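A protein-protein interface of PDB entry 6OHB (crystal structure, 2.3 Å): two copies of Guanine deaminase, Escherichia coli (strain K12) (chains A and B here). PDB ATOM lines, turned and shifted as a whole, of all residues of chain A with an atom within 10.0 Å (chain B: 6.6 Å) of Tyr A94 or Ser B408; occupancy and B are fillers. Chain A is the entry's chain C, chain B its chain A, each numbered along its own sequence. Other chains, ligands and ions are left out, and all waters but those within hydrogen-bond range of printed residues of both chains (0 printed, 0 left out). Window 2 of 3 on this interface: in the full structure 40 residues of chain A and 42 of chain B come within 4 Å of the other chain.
Tyr A94 touches two residues of chain B. Of chain A, only Tyr A94 (3.6 Å) comes within 4 Å of Ser B408. No residue of chain A comes within 4 Å of Val B407. Of chain A, only Tyr A94 (3.6 Å) comes within 4 Å of Val B410. Of the printed residues of chain A, Ser B406 touches Val A91. Printed residues of chain B within 4 Å of Val A91: Ser B406 (3.4 Å) and Asp B411 (3.9998 Å). Of the printed residues of chain B, Leu A305 touches Gln B348 (3.7 Å). Printed residues of chain A within 4 Å of Phe B414: Gly A92 and Ala A93. Trp A101 touches none of the printed residues of chain B. Leu B413 touches none of the printed residues of chain A.
Printed residues of chain A that touch a printed residue of chain B: Val A91, Gly A92, Ala A93, Tyr A94, Gly A95, Tyr A304 and Leu A305. Hydrophobic or aromatic side chains of chain A that line the printed part of chain B: Val A91, Ala A93, Tyr A94 and Tyr A304. Of the 13 printed residues of chain B, 7 touch a printed residue of chain A. Hydrophobic or aromatic side chains of chain B within 4 Å of the printed part of chain A: Tyr B344, Val B410 and Phe B414. Along chain B the printed residues that touch a printed residue of chain A span positions 344 to 414. Among the printed residues, no Asp or Glu carboxylate lies within 4 Å of a Lys or Arg side-chain nitrogen of the other chain.
The side-chain hydroxyl (OH) of Tyr B344 lies close to the backbone NH (N) of Gly A95. The side-chain amide nitrogen (NE2) of Gln B348 sits at hydrogen-bond distance from the backbone carbonyl oxygen (O) of Tyr A304, at 3.0 Å.
No position is printed for both chains. Of the 12 pairs that touch across the chains among the printed residues, none has its exchanged pair printed and touching as well.
Among the printed residues, pairs that only touch across the chains: Val A91 with Ser B406 (3.4 Å), Val A91 with Asp B411 (3.9998 Å), Gly A92 with Phe B414 (3.1 Å), Ala A93 with Asp B411 (3.3 Å), Ala A93 with Phe B414 (3.6 Å), Tyr A94 with Ser B408 (3.6 Å), Tyr A94 with Val B410 (3.6 Å), Gly A95 with Gln B348 (3.8 Å), Tyr A304 with Tyr B344 (3.6 Å) and Leu A305 with Gln B348 (3.7 Å).
O of Ser B406 sits at hydrogen-bond distance from NZ of Lys B412, 3.4 Å away. The side-chain hydroxyl of Ser B408 lies within hydrogen-bond range of the backbone NH of Asp B411 (3.1 Å).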
ATOM      1  N   VAL A  91      -7.409 -16.177  -0.760  1.00  0.00           N
ATOM      2  CA  VAL A  91      -7.466 -17.255  -1.744  1.00  0.00           C
ATOM      3  C   VAL A  91      -8.917 -17.450  -2.162  1.00  0.00           C
ATOM      4  O   VAL A  91      -9.798 -17.624  -1.315  1.00  0.00           O
ATOM      5  CB  VAL A  91      -6.818 -18.558  -1.230  1.00  0.00           C
ATOM      6  CG1 VAL A  91      -5.430 -18.278  -0.710  1.00  0.00           C
ATOM      7  CG2 VAL A  91      -7.642 -19.207  -0.124  1.00  0.00           C
ATOM      8  N   GLY A  92      -9.168 -17.351  -3.463  1.00  0.00           N
ATOM      9  CA  GLY A  92     -10.479 -17.636  -4.017  1.00  0.00           C
ATOM     10  C   GLY A  92     -10.366 -18.741  -5.041  1.00  0.00           C
ATOM     11  O   GLY A  92      -9.953 -18.496  -6.179  1.00  0.00           O
ATOM     12  N   ALA A  93     -10.708 -19.968  -4.649  1.00  0.00           N
ATOM     13  CA  ALA A  93     -10.463 -21.125  -5.499  1.00  0.00           C
ATOM     14  C   ALA A  93     -11.658 -21.521  -6.354  1.00  0.00           C
ATOM     15  O   ALA A  93     -11.477 -22.212  -7.365  1.00  0.00           O
ATOM     16  CB  ALA A  93     -10.045 -22.327  -4.646  1.00  0.00           C
ATOM     17  N   TYR A  94     -12.863 -21.094  -5.987  1.00  0.00           N
ATOM     18  CA  TYR A  94     -14.086 -21.613  -6.584  1.00  0.00           C
ATOM     19  C   TYR A  94     -14.521 -20.838  -7.824  1.00  0.00           C
ATOM     20  O   TYR A  94     -15.712 -20.847  -8.162  1.00  0.00           O
ATOM     21  CB  TYR A  94     -15.194 -21.644  -5.529  1.00  0.00           C
ATOM     22  CG  TYR A  94     -14.802 -22.487  -4.333  1.00  0.00           C
ATOM     23  CD1 TYR A  94     -14.738 -23.875  -4.431  1.00  0.00           C
ATOM     24  CD2 TYR A  94     -14.460 -21.900  -3.119  1.00  0.00           C
ATOM     25  CE1 TYR A  94     -14.366 -24.655  -3.350  1.00  0.00           C
ATOM     26  CE2 TYR A  94     -14.085 -22.676  -2.030  1.00  0.00           C
ATOM     27  CZ  TYR A  94     -14.041 -24.052  -2.152  1.00  0.00           C
ATOM     28  OH  TYR A  94     -13.671 -24.828  -1.075  1.00  0.00           O
ATOM     29  N   GLY A  95     -13.585 -20.184  -8.506  1.00  0.00           N
ATOM     30  CA  GLY A  95     -13.856 -19.562  -9.795  1.00  0.00           C
ATOM     31  C   GLY A  95     -15.001 -18.575  -9.805  1.00  0.00           C
ATOM     32  O   GLY A  95     -15.738 -18.495 -10.794  1.00  0.00           O
ATOM     33  N   GLU A  96     -15.167 -17.816  -8.726  1.00  0.00           N
ATOM     34  CA  GLU A  96     -16.268 -16.871  -8.656  1.00  0.00           C
ATOM     35  C   GLU A  96     -15.994 -15.649  -9.528  1.00  0.00           C
ATOM     36  O   GLU A  96     -14.846 -15.319  -9.844  1.00  0.00           O
ATOM     37  CB  GLU A  96     -16.510 -16.423  -7.213  1.00  0.00           C
ATOM     38  CG  GLU A  96     -16.994 -17.524  -6.288  1.00  0.00           C
ATOM     39  CD  GLU A  96     -18.398 -17.994  -6.610  1.00  0.00           C
ATOM     40  OE1 GLU A  96     -18.852 -18.960  -5.960  1.00  0.00           O
ATOM     41  OE2 GLU A  96     -19.048 -17.407  -7.503  1.00  0.00           O
ATOM     42  N   GLN A  97     -17.075 -14.980  -9.921  1.00  0.00           N
ATOM     43  CA  GLN A  97     -16.990 -13.678 -10.556  1.00  0.00           C
ATOM     44  C   GLN A  97     -17.198 -12.596  -9.496  1.00  0.00           C
ATOM     45  O   GLN A  97     -17.388 -12.885  -8.312  1.00  0.00           O
ATOM     46  CB  GLN A  97     -17.981 -13.576 -11.719  1.00  0.00           C
ATOM     47  CG  GLN A  97     -17.491 -14.323 -12.959  1.00  0.00           C
ATOM     48  CD  GLN A  97     -18.433 -14.215 -14.140  1.00  0.00           C
ATOM     49  OE1 GLN A  97     -19.640 -14.030 -13.975  1.00  0.00           O
ATOM     50  NE2 GLN A  97     -17.885 -14.334 -15.347  1.00  0.00           N
ATOM     51  N   LEU A  98     -17.212 -11.336  -9.946  1.00  0.00           N
ATOM     52  CA  LEU A  98     -16.897 -10.205  -9.073  1.00  0.00           C
ATOM     53  C   LEU A  98     -17.787 -10.147  -7.831  1.00  0.00           C
ATOM     54  O   LEU A  98     -17.280 -10.041  -6.709  1.00  0.00           O
ATOM     55  CB  LEU A  98     -16.988  -8.893  -9.859  1.00  0.00           C
ATOM     56  CG  LEU A  98     -16.751  -7.626  -9.032  1.00  0.00           C
ATOM     57  CD1 LEU A  98     -15.340  -7.606  -8.443  1.00  0.00           C
ATOM     58  CD2 LEU A  98     -17.002  -6.383  -9.868  1.00  0.00           C
ATOM     59  N   GLU A 100     -20.015 -12.329  -6.348  1.00  0.00           N
ATOM     60  CA  GLU A 100     -19.871 -13.471  -5.455  1.00  0.00           C
ATOM     61  C   GLU A 100     -18.474 -13.518  -4.854  1.00  0.00           C
ATOM     62  O   GLU A 100     -18.310 -13.941  -3.705  1.00  0.00           O
ATOM     63  CB  GLU A 100     -20.185 -14.767  -6.200  1.00  0.00           C
ATOM     64  N   TRP A 101     -17.465 -13.084  -5.615  1.00  0.00           N
ATOM     65  CA  TRP A 101     -16.111 -12.975  -5.082  1.00  0.00           C
ATOM     66  C   TRP A 101     -16.063 -12.004  -3.909  1.00  0.00           C
ATOM     67  O   TRP A 101     -15.390 -12.257  -2.904  1.00  0.00           O
ATOM     68  CB  TRP A 101     -15.162 -12.528  -6.195  1.00  0.00           C
ATOM     69  CG  TRP A 101     -13.734 -12.438  -5.785  1.00  0.00           C
ATOM     70  CD1 TRP A 101     -13.146 -11.424  -5.095  1.00  0.00           C
ATOM     71  CD2 TRP A 101     -12.703 -13.400  -6.046  1.00  0.00           C
ATOM     72  NE1 TRP A 101     -11.813 -11.693  -4.905  1.00  0.00           N
ATOM     73  CE2 TRP A 101     -11.516 -12.902  -5.477  1.00  0.00           C
ATOM     74  CE3 TRP A 101     -12.671 -14.636  -6.702  1.00  0.00           C
ATOM     75  CZ2 TRP A 101     -10.306 -13.593  -5.547  1.00  0.00           C
ATOM     76  CZ3 TRP A 101     -11.466 -15.323  -6.770  1.00  0.00           C
ATOM     77  CH2 TRP A 101     -10.303 -14.799  -6.195  1.00  0.00           C
ATOM     78  N   LYS A 104     -17.989 -13.684  -0.848  1.00  0.00           N
ATOM     79  CA  LYS A 104     -17.431 -14.931  -0.342  1.00  0.00           C
ATOM     80  C   LYS A 104     -15.993 -14.794   0.126  1.00  0.00           C
ATOM     81  O   LYS A 104     -15.591 -15.487   1.067  1.00  0.00           O
ATOM     82  CB  LYS A 104     -17.515 -16.025  -1.412  1.00  0.00           C
ATOM     83  N   HIS A 105     -15.211 -13.920  -0.505  1.00  0.00           N
ATOM     84  CA  HIS A 105     -13.777 -13.861  -0.263  1.00  0.00           C
ATOM     85  C   HIS A 105     -13.310 -12.498   0.220  1.00  0.00           C
ATOM     86  O   HIS A 105     -12.588 -12.421   1.221  1.00  0.00           O
ATOM     87  CB  HIS A 105     -13.021 -14.239  -1.551  1.00  0.00           C
ATOM     88  CG  HIS A 105     -13.356 -15.603  -2.073  1.00  0.00           C
ATOM     89  ND1 HIS A 105     -13.359 -16.726  -1.274  1.00  0.00           N
ATOM     90  CD2 HIS A 105     -13.697 -16.024  -3.314  1.00  0.00           C
ATOM     91  CE1 HIS A 105     -13.689 -17.780  -2.000  1.00  0.00           C
ATOM     92  NE2 HIS A 105     -13.897 -17.381  -3.242  1.00  0.00           N
ATOM     93  N   TYR A 304      -8.356 -13.661 -13.833  1.00  0.00           N
ATOM     94  CA  TYR A 304      -8.750 -14.640 -12.818  1.00  0.00           C
ATOM     95  C   TYR A 304     -10.251 -14.618 -12.566  1.00  0.00           C
ATOM     96  O   TYR A 304     -10.867 -15.670 -12.353  1.00  0.00           O
ATOM     97  CB  TYR A 304      -8.017 -14.385 -11.502  1.00  0.00           C
ATOM     98  CG  TYR A 304      -6.660 -15.025 -11.395  1.00  0.00           C
ATOM     99  CD1 TYR A 304      -6.503 -16.399 -11.504  1.00  0.00           C
ATOM    100  CD2 TYR A 304      -5.534 -14.255 -11.149  1.00  0.00           C
ATOM    101  CE1 TYR A 304      -5.255 -16.986 -11.396  1.00  0.00           C
ATOM    102  CE2 TYR A 304      -4.284 -14.829 -11.037  1.00  0.00           C
ATOM    103  CZ  TYR A 304      -4.147 -16.192 -11.161  1.00  0.00           C
ATOM    104  OH  TYR A 304      -2.894 -16.754 -11.045  1.00  0.00           O
ATOM    105  N   LEU A 305     -10.853 -13.434 -12.566  1.00  0.00           N
ATOM    106  CA  LEU A 305     -12.281 -13.297 -12.325  1.00  0.00           C
ATOM    107  C   LEU A 305     -13.096 -13.346 -13.607  1.00  0.00           C
ATOM    108  O   LEU A 305     -14.324 -13.231 -13.543  1.00  0.00           O
ATOM    109  CB  LEU A 305     -12.574 -11.987 -11.584  1.00  0.00           C
ATOM    110  CG  LEU A 305     -12.405 -11.928 -10.060  1.00  0.00           C
ATOM    111  CD1 LEU A 305     -11.224 -12.753  -9.549  1.00  0.00           C
ATOM    112  CD2 LEU A 305     -12.281 -10.477  -9.610  1.00  0.00           C
ATOM    113  N   TYR B 344      -5.938 -22.080 -16.048  1.00  0.00           N
ATOM    114  CA  TYR B 344      -7.029 -21.530 -15.256  1.00  0.00           C
ATOM    115  C   TYR B 344      -7.485 -20.179 -15.806  1.00  0.00           C
ATOM    116  O   TYR B 344      -8.691 -19.912 -15.888  1.00  0.00           O
ATOM    117  CB  TYR B 344      -6.596 -21.412 -13.793  1.00  0.00           C
ATOM    118  CG  TYR B 344      -7.681 -20.901 -12.877  1.00  0.00           C
ATOM    119  CD1 TYR B 344      -7.874 -19.532 -12.683  1.00  0.00           C
ATOM    120  CD2 TYR B 344      -8.519 -21.783 -12.207  1.00  0.00           C
ATOM    121  CE1 TYR B 344      -8.876 -19.059 -11.846  1.00  0.00           C
ATOM    122  CE2 TYR B 344      -9.522 -21.321 -11.367  1.00  0.00           C
ATOM    123  CZ  TYR B 344      -9.697 -19.961 -11.192  1.00  0.00           C
ATOM    124  OH  TYR B 344     -10.692 -19.505 -10.356  1.00  0.00           O
ATOM    125  N   GLN B 348     -11.153 -19.457 -17.340  1.00  0.00           N
ATOM    126  CA  GLN B 348     -11.970 -18.379 -16.789  1.00  0.00           C
ATOM    127  C   GLN B 348     -12.446 -17.449 -17.895  1.00  0.00           C
ATOM    128  O   GLN B 348     -13.573 -16.941 -17.853  1.00  0.00           O
ATOM    129  CB  GLN B 348     -11.184 -17.587 -15.743  1.00  0.00           C
ATOM    130  CG  GLN B 348     -11.242 -18.149 -14.331  1.00  0.00           C
ATOM    131  CD  GLN B 348     -12.647 -18.180 -13.757  1.00  0.00           C
ATOM    132  OE1 GLN B 348     -13.190 -19.251 -13.476  1.00  0.00           O
ATOM    133  NE2 GLN B 348     -13.252 -17.007 -13.602  1.00  0.00           N
ATOM    134  N   ARG B 353     -14.760 -23.160 -15.093  1.00  0.00           N
ATOM    135  CA  ARG B 353     -14.044 -23.134 -13.821  1.00  0.00           C
ATOM    136  C   ARG B 353     -13.168 -24.377 -13.729  1.00  0.00           C
ATOM    137  O   ARG B 353     -13.677 -25.499 -13.632  1.00  0.00           O
ATOM    138  CB  ARG B 353     -15.018 -23.056 -12.648  1.00  0.00           C
ATOM    139  N   TYR B 357      -8.739 -29.966  -8.100  1.00  0.00           N
ATOM    140  CA  TYR B 357      -8.659 -31.399  -8.356  1.00  0.00           C
ATOM    141  C   TYR B 357      -8.429 -31.681  -9.835  1.00  0.00           C
ATOM    142  O   TYR B 357      -7.603 -32.531 -10.187  1.00  0.00           O
ATOM    143  CB  TYR B 357      -9.930 -32.086  -7.854  1.00  0.00           C
ATOM    144  CG  TYR B 357     -10.033 -32.107  -6.344  1.00  0.00           C
ATOM    145  CD1 TYR B 357      -8.943 -31.768  -5.552  1.00  0.00           C
ATOM    146  CD2 TYR B 357     -11.219 -32.449  -5.712  1.00  0.00           C
ATOM    147  CE1 TYR B 357      -9.027 -31.778  -4.175  1.00  0.00           C
ATOM    148  CE2 TYR B 357     -11.313 -32.459  -4.331  1.00  0.00           C
ATOM    149  CZ  TYR B 357     -10.213 -32.130  -3.568  1.00  0.00           C
ATOM    150  OH  TYR B 357     -10.297 -32.133  -2.193  1.00  0.00           O
ATOM    151  N   SER B 406      -5.721 -21.090   4.255  1.00  0.00           N
ATOM    152  CA  SER B 406      -6.585 -22.006   3.534  1.00  0.00           C
ATOM    153  C   SER B 406      -7.014 -23.133   4.459  1.00  0.00           C
ATOM    154  O   SER B 406      -6.196 -23.697   5.190  1.00  0.00           O
ATOM    155  CB  SER B 406      -5.874 -22.570   2.305  1.00  0.00           C
ATOM    156  OG  SER B 406      -5.627 -21.555   1.347  1.00  0.00           O
ATOM    157  N   VAL B 407      -8.298 -23.466   4.422  1.00  0.00           N
ATOM    158  CA  VAL B 407      -8.841 -24.503   5.290  1.00  0.00           C
ATOM    159  C   VAL B 407      -9.044 -25.816   4.545  1.00  0.00           C
ATOM    160  O   VAL B 407      -8.761 -26.884   5.089  1.00  0.00           O
ATOM    161  CB  VAL B 407     -10.155 -24.025   5.944  1.00  0.00           C
ATOM    162  CG1 VAL B 407      -9.849 -23.145   7.151  1.00  0.00           C
ATOM    163  CG2 VAL B 407     -11.025 -23.279   4.935  1.00  0.00           C
ATOM    164  N   SER B 408      -9.506 -25.761   3.302  1.00  0.00           N
ATOM    165  CA  SER B 408      -9.760 -26.962   2.520  1.00  0.00           C
ATOM    166  C   SER B 408      -8.536 -27.358   1.697  1.00  0.00           C
ATOM    167  O   SER B 408      -7.633 -26.556   1.447  1.00  0.00           O
ATOM    168  CB  SER B 408     -10.966 -26.756   1.609  1.00  0.00           C
ATOM    169  OG  SER B 408     -10.597 -26.021   0.461  1.00  0.00           O
ATOM    170  N   LEU B 409      -8.512 -28.633   1.292  1.00  0.00           N
ATOM    171  CA  LEU B 409      -7.415 -29.145   0.475  1.00  0.00           C
ATOM    172  C   LEU B 409      -7.410 -28.514  -0.911  1.00  0.00           C
ATOM    173  O   LEU B 409      -6.336 -28.271  -1.482  1.00  0.00           O
ATOM    174  CB  LEU B 409      -7.502 -30.669   0.374  1.00  0.00           C
ATOM    175  CG  LEU B 409      -6.488 -31.375  -0.531  1.00  0.00           C
ATOM    176  CD1 LEU B 409      -5.055 -31.077  -0.096  1.00  0.00           C
ATOM    177  CD2 LEU B 409      -6.739 -32.876  -0.530  1.00  0.00           C
ATOM    178  N   VAL B 410      -8.595 -28.255  -1.478  1.00  0.00           N
ATOM    179  CA  VAL B 410      -8.653 -27.602  -2.784  1.00  0.00           C
ATOM    180  C   VAL B 410      -8.050 -26.208  -2.701  1.00  0.00           C
ATOM    181  O   VAL B 410      -7.396 -25.742  -3.641  1.00  0.00           O
ATOM    182  CB  VAL B 410     -10.099 -27.563  -3.325  1.00  0.00           C
ATOM    183  CG1 VAL B 410     -10.746 -28.918  -3.218  1.00  0.00           C
ATOM    184  CG2 VAL B 410     -10.945 -26.510  -2.615  1.00  0.00           C
ATOM    185  N   ASP B 411      -8.249 -25.527  -1.570  1.00  0.00           N
ATOM    186  CA  ASP B 411      -7.632 -24.223  -1.363  1.00  0.00           C
ATOM    187  C   ASP B 411      -6.112 -24.328  -1.362  1.00  0.00           C
ATOM    188  O   ASP B 411      -5.425 -23.477  -1.939  1.00  0.00           O
ATOM    189  CB  ASP B 411      -8.140 -23.609  -0.057  1.00  0.00           C
ATOM    190  CG  ASP B 411      -9.450 -22.859  -0.230  1.00  0.00           C
ATOM    191  OD1 ASP B 411      -9.954 -22.786  -1.371  1.00  0.00           O
ATOM    192  OD2 ASP B 411      -9.972 -22.331   0.776  1.00  0.00           O
ATOM    193  N   LYS B 412      -5.565 -25.359  -0.711  1.00  0.00           N
ATOM    194  CA  LYS B 412      -4.114 -25.526  -0.676  1.00  0.00           C
ATOM    195  C   LYS B 412      -3.555 -25.844  -2.062  1.00  0.00           C
ATOM    196  O   LYS B 412      -2.520 -25.291  -2.464  1.00  0.00           O
ATOM    197  CB  LYS B 412      -3.746 -26.602   0.349  1.00  0.00           C
ATOM    198  CG  LYS B 412      -4.191 -26.243   1.773  1.00  0.00           C
ATOM    199  CD  LYS B 412      -3.891 -27.347   2.778  1.00  0.00           C
ATOM    200  CE  LYS B 412      -4.390 -26.987   4.180  1.00  0.00           C
ATOM    201  NZ  LYS B 412      -3.630 -25.871   4.824  1.00  0.00           N
ATOM    202  N   LEU B 413      -4.238 -26.710  -2.815  1.00  0.00           N
ATOM    203  CA  LEU B 413      -3.820 -26.978  -4.190  1.00  0.00           C
ATOM    204  C   LEU B 413      -3.892 -25.714  -5.041  1.00  0.00           C
ATOM    205  O   LEU B 413      -3.025 -25.475  -5.889  1.00  0.00           O
ATOM    206  CB  LEU B 413      -4.686 -28.079  -4.800  1.00  0.00           C
ATOM    207  CG  LEU B 413      -4.458 -29.520  -4.333  1.00  0.00           C
ATOM    208  CD1 LEU B 413      -5.430 -30.455  -5.032  1.00  0.00           C
ATOM    209  CD2 LEU B 413      -3.020 -29.944  -4.604  1.00  0.00           C
ATOM    210  N   PHE B 414      -4.920 -24.891  -4.824  1.00  0.00           N
ATOM    211  CA  PHE B 414      -5.056 -23.651  -5.576  1.00  0.00           C
ATOM    212  C   PHE B 414      -3.928 -22.680  -5.244  1.00  0.00           C
ATOM    213  O   PHE B 414      -3.403 -22.003  -6.136  1.00  0.00           O
ATOM    214  CB  PHE B 414      -6.424 -23.027  -5.291  1.00  0.00           C
ATOM    215  CG  PHE B 414      -6.774 -21.889  -6.202  1.00  0.00           C
ATOM    216  CD1 PHE B 414      -7.198 -22.131  -7.499  1.00  0.00           C
ATOM    217  CD2 PHE B 414      -6.684 -20.575  -5.761  1.00  0.00           C
ATOM    218  CE1 PHE B 414      -7.524 -21.086  -8.348  1.00  0.00           C
ATOM    219  CE2 PHE B 414      -7.006 -19.521  -6.603  1.00  0.00           C
ATOM    220  CZ  PHE B 414      -7.427 -19.776  -7.899  1.00  0.00           C
